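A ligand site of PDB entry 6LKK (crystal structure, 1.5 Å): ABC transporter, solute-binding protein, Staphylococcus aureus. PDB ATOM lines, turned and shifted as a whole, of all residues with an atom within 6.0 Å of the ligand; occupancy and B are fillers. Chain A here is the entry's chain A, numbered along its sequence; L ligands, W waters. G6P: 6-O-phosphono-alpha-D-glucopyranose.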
ATOM      1  N   SER A   7       6.148   0.076 -29.779  1.00  0.00           N
ATOM      2  CA  SER A   7       5.204   0.172 -28.674  1.00  0.00           C
ATOM      3  C   SER A   7       4.954   1.604 -28.219  1.00  0.00           C
ATOM      4  O   SER A   7       5.900   2.359 -28.001  1.00  0.00           O
ATOM      5  CB  SER A   7       5.692  -0.648 -27.477  1.00  0.00           C
ATOM      6  OG  SER A   7       4.760  -0.568 -26.426  1.00  0.00           O
ATOM      7  N   PRO A   8       3.689   2.012 -28.049  1.00  0.00           N
ATOM      8  CA  PRO A   8       3.410   3.293 -27.396  1.00  0.00           C
ATOM      9  C   PRO A   8       3.523   3.254 -25.886  1.00  0.00           C
ATOM     10  O   PRO A   8       3.408   4.315 -25.246  1.00  0.00           O
ATOM     11  CB  PRO A   8       1.959   3.589 -27.824  1.00  0.00           C
ATOM     12  CG  PRO A   8       1.363   2.243 -27.981  1.00  0.00           C
ATOM     13  CD  PRO A   8       2.458   1.379 -28.563  1.00  0.00           C
ATOM     14  N   TYR A   9       3.739   2.090 -25.288  1.00  0.00           N
ATOM     15  CA  TYR A   9       3.915   2.013 -23.838  1.00  0.00           C
ATOM     16  C   TYR A   9       5.144   2.801 -23.407  1.00  0.00           C
ATOM     17  O   TYR A   9       6.101   2.972 -24.165  1.00  0.00           O
ATOM     18  CB  TYR A   9       4.079   0.570 -23.365  1.00  0.00           C
ATOM     19  CG  TYR A   9       2.830  -0.280 -23.421  1.00  0.00           C
ATOM     20  CD1 TYR A   9       1.694   0.078 -22.708  1.00  0.00           C
ATOM     21  CD2 TYR A   9       2.804  -1.463 -24.148  1.00  0.00           C
ATOM     22  CE1 TYR A   9       0.553  -0.708 -22.748  1.00  0.00           C
ATOM     23  CE2 TYR A   9       1.675  -2.254 -24.183  1.00  0.00           C
ATOM     24  CZ  TYR A   9       0.549  -1.872 -23.489  1.00  0.00           C
ATOM     25  OH  TYR A   9      -0.576  -2.655 -23.527  1.00  0.00           O
ATOM     26  N   GLN A  10       5.111   3.266 -22.171  1.00  0.00           N
ATOM     27  CA  GLN A  10       6.300   3.852 -21.560  1.00  0.00           C
ATOM     28  C   GLN A  10       7.290   2.751 -21.185  1.00  0.00           C
ATOM     29  O   GLN A  10       6.906   1.615 -20.891  1.00  0.00           O
ATOM     30  CB  GLN A  10       5.922   4.669 -20.323  1.00  0.00           C
ATOM     31  CG  GLN A  10       5.103   5.906 -20.652  1.00  0.00           C
ATOM     32  CD  GLN A  10       5.848   6.898 -21.523  1.00  0.00           C
ATOM     33  OE1 GLN A  10       6.797   7.532 -21.072  1.00  0.00           O
ATOM     34  NE2 GLN A  10       5.430   7.015 -22.781  1.00  0.00           N
ATOM     35  N   GLY A  34       6.717   5.718 -29.405  1.00  0.00           N
ATOM     36  CA  GLY A  34       6.025   6.805 -30.064  1.00  0.00           C
ATOM     37  C   GLY A  34       4.544   6.700 -29.833  1.00  0.00           C
ATOM     38  O   GLY A  34       4.033   5.717 -29.291  1.00  0.00           O
ATOM     39  N   SER A  35       3.843   7.757 -30.241  1.00  0.00           N
ATOM     40  CA  SER A  35       2.390   7.726 -30.216  1.00  0.00           C
ATOM     41  C   SER A  35       1.885   6.601 -31.111  1.00  0.00           C
ATOM     42  O   SER A  35       2.503   6.261 -32.119  1.00  0.00           O
ATOM     43  CB  SER A  35       1.813   9.068 -30.683  1.00  0.00           C
ATOM     44  OG  SER A  35       2.246  10.115 -29.848  1.00  0.00           O
ATOM     45  N   THR A  36       0.750   5.998 -30.715  1.00  0.00           N
ATOM     46  CA  THR A  36       0.273   4.792 -31.392  1.00  0.00           C
ATOM     47  C   THR A  36       0.173   4.998 -32.902  1.00  0.00           C
ATOM     48  O   THR A  36       0.739   4.222 -33.681  1.00  0.00           O
ATOM     49  CB  THR A  36      -1.097   4.376 -30.835  1.00  0.00           C
ATOM     50  OG1 THR A  36      -0.995   4.091 -29.429  1.00  0.00           O
ATOM     51  CG2 THR A  36      -1.607   3.139 -31.549  1.00  0.00           C
ATOM     52  N   GLN A  37      -0.542   6.032 -33.324  1.00  0.00           N
ATOM     53  CA  GLN A  37      -0.774   6.215 -34.754  1.00  0.00           C
ATOM     54  C   GLN A  37       0.467   6.695 -35.480  1.00  0.00           C
ATOM     55  O   GLN A  37       0.634   6.425 -36.673  1.00  0.00           O
ATOM     56  CB  GLN A  37      -1.933   7.183 -34.977  1.00  0.00           C
ATOM     57  CG  GLN A  37      -3.288   6.632 -34.543  1.00  0.00           C
ATOM     58  CD  GLN A  37      -3.639   5.346 -35.258  1.00  0.00           C
ATOM     59  OE1 GLN A  37      -3.468   5.228 -36.469  1.00  0.00           O
ATOM     60  NE2 GLN A  37      -4.118   4.363 -34.513  1.00  0.00           N
ATOM     61  N   MET A  56       3.200  -3.881 -29.891  1.00  0.00           N
ATOM     62  CA  MET A  56       2.476  -4.142 -28.653  1.00  0.00           C
ATOM     63  C   MET A  56       2.036  -2.832 -28.021  1.00  0.00           C
ATOM     64  O   MET A  56       2.818  -1.885 -27.921  1.00  0.00           O
ATOM     65  CB  MET A  56       3.332  -4.948 -27.655  1.00  0.00           C
ATOM     66  CG  MET A  56       4.507  -4.206 -27.051  1.00  0.00           C
ATOM     67  SD  MET A  56       5.490  -5.265 -25.960  1.00  0.00           S
ATOM     68  CE  MET A  56       4.395  -5.465 -24.557  1.00  0.00           C
ATOM     69  N   GLY A  57       0.772  -2.788 -27.610  1.00  0.00           N
ATOM     70  CA  GLY A  57       0.190  -1.594 -27.053  1.00  0.00           C
ATOM     71  C   GLY A  57      -0.725  -0.882 -28.036  1.00  0.00           C
ATOM     72  O   GLY A  57      -0.653  -1.078 -29.255  1.00  0.00           O
ATOM     73  N   GLY A  58      -1.596  -0.049 -27.495  1.00  0.00           N
ATOM     74  CA  GLY A  58      -2.626   0.585 -28.290  1.00  0.00           C
ATOM     75  C   GLY A  58      -3.797  -0.342 -28.542  1.00  0.00           C
ATOM     76  O   GLY A  58      -3.727  -1.565 -28.380  1.00  0.00           O
ATOM     77  N   VAL A  59      -4.911   0.257 -28.936  1.00  0.00           N
ATOM     78  CA  VAL A  59      -6.133  -0.489 -29.220  1.00  0.00           C
ATOM     79  C   VAL A  59      -6.057  -0.986 -30.656  1.00  0.00           C
ATOM     80  O   VAL A  59      -6.803  -0.551 -31.536  1.00  0.00           O
ATOM     81  CB  VAL A  59      -7.400   0.364 -28.966  1.00  0.00           C
ATOM     82  CG1 VAL A  59      -7.545   0.604 -27.470  1.00  0.00           C
ATOM     83  CG2 VAL A  59      -7.334   1.691 -29.714  1.00  0.00           C
ATOM     84  N   MET A  98      -6.730  -1.620 -20.221  1.00  0.00           N
ATOM     85  CA  MET A  98      -6.212  -0.331 -19.769  1.00  0.00           C
ATOM     86  C   MET A  98      -7.354   0.670 -19.665  1.00  0.00           C
ATOM     87  O   MET A  98      -7.790   1.229 -20.688  1.00  0.00           O
ATOM     88  CB  MET A  98      -5.131   0.190 -20.703  1.00  0.00           C
ATOM     89  CG  MET A  98      -4.376   1.392 -20.160  1.00  0.00           C
ATOM     90  SD  MET A  98      -3.325   0.961 -18.763  1.00  0.00           S
ATOM     91  CE  MET A  98      -2.047   0.060 -19.618  1.00  0.00           C
ATOM     92  N   THR A 100      -8.954   4.173 -19.401  1.00  0.00           N
ATOM     93  CA  THR A 100      -8.620   5.577 -19.507  1.00  0.00           C
ATOM     94  C   THR A 100      -9.155   6.294 -18.267  1.00  0.00           C
ATOM     95  O   THR A 100     -10.130   5.864 -17.656  1.00  0.00           O
ATOM     96  CB  THR A 100      -9.209   6.194 -20.779  1.00  0.00           C
ATOM     97  OG1 THR A 100     -10.633   6.053 -20.768  1.00  0.00           O
ATOM     98  CG2 THR A 100      -8.647   5.488 -22.013  1.00  0.00           C
ATOM     99  N   SER A 132      -4.367  14.781 -25.053  1.00  0.00           N
ATOM    100  CA  SER A 132      -3.444  14.525 -26.154  1.00  0.00           C
ATOM    101  C   SER A 132      -4.183  14.380 -27.480  1.00  0.00           C
ATOM    102  O   SER A 132      -5.366  14.048 -27.540  1.00  0.00           O
ATOM    103  CB  SER A 132      -2.596  13.274 -25.877  1.00  0.00           C
ATOM    104  OG  SER A 132      -3.391  12.151 -25.568  1.00  0.00           O
ATOM    105  N   THR A 136      -3.405  11.288 -33.380  1.00  0.00           N
ATOM    106  CA  THR A 136      -2.146  10.553 -33.352  1.00  0.00           C
ATOM    107  C   THR A 136      -2.006   9.593 -32.174  1.00  0.00           C
ATOM    108  O   THR A 136      -1.102   8.755 -32.209  1.00  0.00           O
ATOM    109  CB  THR A 136      -0.966  11.529 -33.305  1.00  0.00           C
ATOM    110  OG1 THR A 136      -1.098  12.409 -32.182  1.00  0.00           O
ATOM    111  CG2 THR A 136      -0.885  12.346 -34.588  1.00  0.00           C
ATOM    112  N   THR A 137      -2.860   9.685 -31.158  1.00  0.00           N
ATOM    113  CA  THR A 137      -2.684   8.907 -29.937  1.00  0.00           C
ATOM    114  C   THR A 137      -3.892   8.017 -29.689  1.00  0.00           C
ATOM    115  O   THR A 137      -5.033   8.359 -30.048  1.00  0.00           O
ATOM    116  CB  THR A 137      -2.478   9.814 -28.717  1.00  0.00           C
ATOM    117  OG1 THR A 137      -3.667  10.562 -28.448  1.00  0.00           O
ATOM    118  CG2 THR A 137      -1.310  10.768 -28.930  1.00  0.00           C
ATOM    119  N   THR A 138      -3.650   6.861 -29.060  1.00  0.00           N
ATOM    120  CA  THR A 138      -4.752   6.050 -28.574  1.00  0.00           C
ATOM    121  C   THR A 138      -5.527   6.771 -27.480  1.00  0.00           C
ATOM    122  O   THR A 138      -6.760   6.770 -27.471  1.00  0.00           O
ATOM    123  CB  THR A 138      -4.216   4.712 -28.036  1.00  0.00           C
ATOM    124  OG1 THR A 138      -3.756   3.896 -29.112  1.00  0.00           O
ATOM    125  CG2 THR A 138      -5.310   3.948 -27.263  1.00  0.00           C
ATOM    126  N   THR A 139      -4.805   7.401 -26.552  1.00  0.00           N
ATOM    127  CA  THR A 139      -5.442   7.942 -25.351  1.00  0.00           C
ATOM    128  C   THR A 139      -6.371   9.100 -25.706  1.00  0.00           C
ATOM    129  O   THR A 139      -7.524   9.127 -25.255  1.00  0.00           O
ATOM    130  CB  THR A 139      -4.374   8.395 -24.359  1.00  0.00           C
ATOM    131  OG1 THR A 139      -3.528   7.271 -24.049  1.00  0.00           O
ATOM    132  CG2 THR A 139      -5.011   8.895 -23.075  1.00  0.00           C
ATOM    133  N   GLY A 140      -5.902  10.057 -26.503  1.00  0.00           N
ATOM    134  CA  GLY A 140      -6.765  11.149 -26.919  1.00  0.00           C
ATOM    135  C   GLY A 140      -7.967  10.664 -27.700  1.00  0.00           C
ATOM    136  O   GLY A 140      -9.100  11.093 -27.458  1.00  0.00           O
ATOM    137  N   GLN A 142      -9.429   7.675 -27.622  1.00  0.00           N
ATOM    138  CA  GLN A 142     -10.361   6.931 -26.796  1.00  0.00           C
ATOM    139  C   GLN A 142     -11.162   7.867 -25.890  1.00  0.00           C
ATOM    140  O   GLN A 142     -12.359   7.644 -25.665  1.00  0.00           O
ATOM    141  CB  GLN A 142      -9.606   5.885 -25.966  1.00  0.00           C
ATOM    142  CG  GLN A 142      -9.066   4.722 -26.789  1.00  0.00           C
ATOM    143  CD  GLN A 142     -10.174   3.852 -27.362  1.00  0.00           C
ATOM    144  OE1 GLN A 142     -10.666   4.092 -28.460  1.00  0.00           O
ATOM    145  NE2 GLN A 142     -10.569   2.815 -26.619  1.00  0.00           N
ATOM    146  N   LYS A 169       1.651  14.764 -27.051  1.00  0.00           N
ATOM    147  CA  LYS A 169       2.029  13.467 -26.501  1.00  0.00           C
ATOM    148  C   LYS A 169       1.185  13.141 -25.271  1.00  0.00           C
ATOM    149  O   LYS A 169       1.029  13.981 -24.378  1.00  0.00           O
ATOM    150  CB  LYS A 169       3.510  13.451 -26.133  1.00  0.00           C
ATOM    151  CG  LYS A 169       4.453  13.702 -27.305  1.00  0.00           C
ATOM    152  CD  LYS A 169       4.406  12.584 -28.336  1.00  0.00           C
ATOM    153  CE  LYS A 169       4.855  11.260 -27.746  1.00  0.00           C
ATOM    154  NZ  LYS A 169       5.676  10.466 -28.702  1.00  0.00           N
ATOM    155  N   THR A 170       0.663  11.914 -25.230  1.00  0.00           N
ATOM    156  CA  THR A 170      -0.122  11.465 -24.091  1.00  0.00           C
ATOM    157  C   THR A 170       0.642  11.614 -22.780  1.00  0.00           C
ATOM    158  O   THR A 170       0.080  12.055 -21.773  1.00  0.00           O
ATOM    159  CB  THR A 170      -0.548  10.017 -24.302  1.00  0.00           C
ATOM    160  OG1 THR A 170      -1.415   9.937 -25.447  1.00  0.00           O
ATOM    161  CG2 THR A 170      -1.285   9.470 -23.084  1.00  0.00           C
ATOM    162  N   SER A 171       1.919  11.233 -22.771  1.00  0.00           N
ATOM    163  CA  SER A 171       2.667  11.269 -21.517  1.00  0.00           C
ATOM    164  C   SER A 171       2.979  12.687 -21.062  1.00  0.00           C
ATOM    165  O   SER A 171       3.266  12.892 -19.885  1.00  0.00           O
ATOM    166  CB  SER A 171       3.954  10.454 -21.644  1.00  0.00           C
ATOM    167  OG  SER A 171       3.668   9.058 -21.567  1.00  0.00           O
ATOM    168  N   SER A 187      -5.799  10.973 -19.354  1.00  0.00           N
ATOM    169  CA  SER A 187      -4.640  10.081 -19.343  1.00  0.00           C
ATOM    170  C   SER A 187      -5.135   8.641 -19.360  1.00  0.00           C
ATOM    171  O   SER A 187      -6.261   8.345 -19.771  1.00  0.00           O
ATOM    172  CB  SER A 187      -3.746  10.405 -18.138  1.00  0.00           C
ATOM    173  OG  SER A 187      -2.609   9.566 -18.092  1.00  0.00           O
ATOM    174  N   TYR A 188      -4.278   7.719 -18.933  1.00  0.00           N
ATOM    175  CA  TYR A 188      -4.668   6.326 -18.792  1.00  0.00           C
ATOM    176  C   TYR A 188      -4.053   5.770 -17.515  1.00  0.00           C
ATOM    177  O   TYR A 188      -3.108   6.339 -16.954  1.00  0.00           O
ATOM    178  CB  TYR A 188      -4.275   5.481 -20.014  1.00  0.00           C
ATOM    179  CG  TYR A 188      -2.788   5.397 -20.303  1.00  0.00           C
ATOM    180  CD1 TYR A 188      -2.148   6.396 -21.041  1.00  0.00           C
ATOM    181  CD2 TYR A 188      -2.038   4.317 -19.877  1.00  0.00           C
ATOM    182  CE1 TYR A 188      -0.796   6.314 -21.318  1.00  0.00           C
ATOM    183  CE2 TYR A 188      -0.679   4.229 -20.158  1.00  0.00           C
ATOM    184  CZ  TYR A 188      -0.070   5.230 -20.877  1.00  0.00           C
ATOM    185  OH  TYR A 188       1.270   5.154 -21.159  1.00  0.00           O
ATOM    186  N   ASN A 214      -9.686   0.412 -22.667  1.00  0.00           N
ATOM    187  CA  ASN A 214      -8.880   0.013 -23.810  1.00  0.00           C
ATOM    188  C   ASN A 214      -8.511  -1.451 -23.694  1.00  0.00           C
ATOM    189  O   ASN A 214      -8.033  -1.905 -22.652  1.00  0.00           O
ATOM    190  CB  ASN A 214      -7.601   0.847 -23.901  1.00  0.00           C
ATOM    191  CG  ASN A 214      -7.876   2.327 -24.051  1.00  0.00           C
ATOM    192  OD1 ASN A 214      -8.990   2.741 -24.346  1.00  0.00           O
ATOM    193  ND2 ASN A 214      -6.836   3.133 -23.869  1.00  0.00           N
ATOM    194  N   ASP A 216      -5.774  -3.388 -25.021  1.00  0.00           N
ATOM    195  CA  ASP A 216      -4.484  -3.304 -25.696  1.00  0.00           C
ATOM    196  C   ASP A 216      -4.178  -4.621 -26.399  1.00  0.00           C
ATOM    197  O   ASP A 216      -4.542  -5.701 -25.932  1.00  0.00           O
ATOM    198  CB  ASP A 216      -3.384  -2.968 -24.698  1.00  0.00           C
ATOM    199  CG  ASP A 216      -3.535  -1.581 -24.079  1.00  0.00           C
ATOM    200  OD1 ASP A 216      -4.462  -0.842 -24.483  1.00  0.00           O
ATOM    201  OD2 ASP A 216      -2.718  -1.242 -23.202  1.00  0.00           O
HETATM  202  C1  G6P L   1      -3.387   4.024 -24.547  1.00  0.00           C
HETATM  203  C2  G6P L   1      -3.198   2.487 -24.485  1.00  0.00           C
HETATM  204  C3  G6P L   1      -1.812   2.046 -24.178  1.00  0.00           C
HETATM  205  C4  G6P L   1      -0.830   2.922 -24.815  1.00  0.00           C
HETATM  206  C5  G6P L   1      -0.890   4.304 -24.157  1.00  0.00           C
HETATM  207  C6  G6P L   1      -0.008   5.271 -24.877  1.00  0.00           C
HETATM  208  O1  G6P L   1      -4.448   4.414 -23.729  1.00  0.00           O
HETATM  209  O2  G6P L   1      -4.079   1.927 -23.495  1.00  0.00           O
HETATM  210  O3  G6P L   1      -1.638   0.657 -24.705  1.00  0.00           O
HETATM  211  O4  G6P L   1       0.512   2.396 -24.631  1.00  0.00           O
HETATM  212  O5  G6P L   1      -2.251   4.874 -24.167  1.00  0.00           O
HETATM  213  O6  G6P L   1      -0.404   5.325 -26.228  1.00  0.00           O
HETATM  214  P   G6P L   1      -0.669   6.833 -26.945  1.00  0.00           P
HETATM  215  O1P G6P L   1      -0.960   6.602 -28.412  1.00  0.00           O
HETATM  216  O2P G6P L   1       0.585   7.720 -26.789  1.00  0.00           O
HETATM  217  O3P G6P L   1      -1.841   7.497 -26.300  1.00  0.00           O
HETATM  218  O   HOH W   1       2.906   6.838 -25.786  1.00  0.00           O
HETATM  219  O   HOH W   2       1.667   9.983 -27.192  1.00  0.00           O
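An oxygen (O1P) of the ligand lies within hydrogen-bond range of the side-chain hydroxyl (OG1) of Thr 36 (2.7 Å). O3P of the ligand is in hydrogen-bond range of N of Thr 139 (3.0 Å). OG1 of Thr 170 is in hydrogen-bond range of O3P of the ligand (2.6 Å). An oxygen (O1P) of the ligand lies within hydrogen-bond range of the backbone NH (N) of Thr 138, 2.8 Å away. An oxygen (O1P) of the ligand lies within hydrogen-bond range of the backbone NH (N) of Thr 36 (2.9 Å). The side-chain amide nitrogen (ND2) of Asn 214 sits at hydrogen-bond distance from an oxygen (O1) of the ligand, 2.7 Å away. An oxygen (O4) of the ligand lies close to the backbone NH (N) of Tyr 9, at 3.3 Å. O3 of the ligand sits at hydrogen-bond distance from OD2 of Asp 216 (2.7 Å). N of Gly 58 sits at hydrogen-bond distance from O3 of the ligand, at 2.9 Å. O5 of the ligand lies within hydrogen-bond range of OG1 of Thr 139, 2.7 Å away.
OD1 of Asn 214 is in hydrogen-bond range of NE2 of Gln 142, at 2.8 Å. O of Asn 214 lies within hydrogen-bond range of N of Met 98. The side-chain hydroxyl (OG1) of Thr 137 sits at hydrogen-bond distance from the backbone NH (N) of Gly 140, 3.0 Å away. The side-chain carboxylate (OD2) of Asp 216 lies within hydrogen-bond range of the side-chain hydroxyl (OH) of Tyr 9 (2.6 Å). OG of Ser 7 sits at hydrogen-bond distance from N of Tyr 9 (3.1 Å). The side-chain hydroxyl (OG) of Ser 132 lies within hydrogen-bond range of the side-chain hydroxyl (OG1) of Thr 137 (3.3 Å). OG1 of Thr 36 lies within hydrogen-bond range of OG1 of Thr 138, at 2.8 Å. OG1 of Thr 170 sits at hydrogen-bond distance from OG of Ser 132, at 3.0 Å.
Pro 8 touches the ligand. Ser 35 touches the ligand (CA to O2P, 3.9 Å). Gly 57 touches the ligand. Met 98 touches the ligand (CG to O2, 3.4 Å). CA of Thr 137 touches O1P of the ligand, at 3.3 Å. CD1 of Tyr 188 touches O5 of the ligand, at 3.5 Å. Of the 28 residues printed, 14 come within 4 Å of the ligand. Along chain A the residues within 4 Å of the ligand span positions 8 to 216. The nearest printed residue that does not touch the ligand is Thr 136 (4.4 Å).
Water W2 lies within hydrogen-bond range of O2P of the ligand (2.5 Å), OG of Ser 35 (2.7 Å) and N of Thr 170 (2.9 Å). Water W1 bridges O of Pro 8 (2.6 Å) and O2P of the ligand (2.7 Å).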
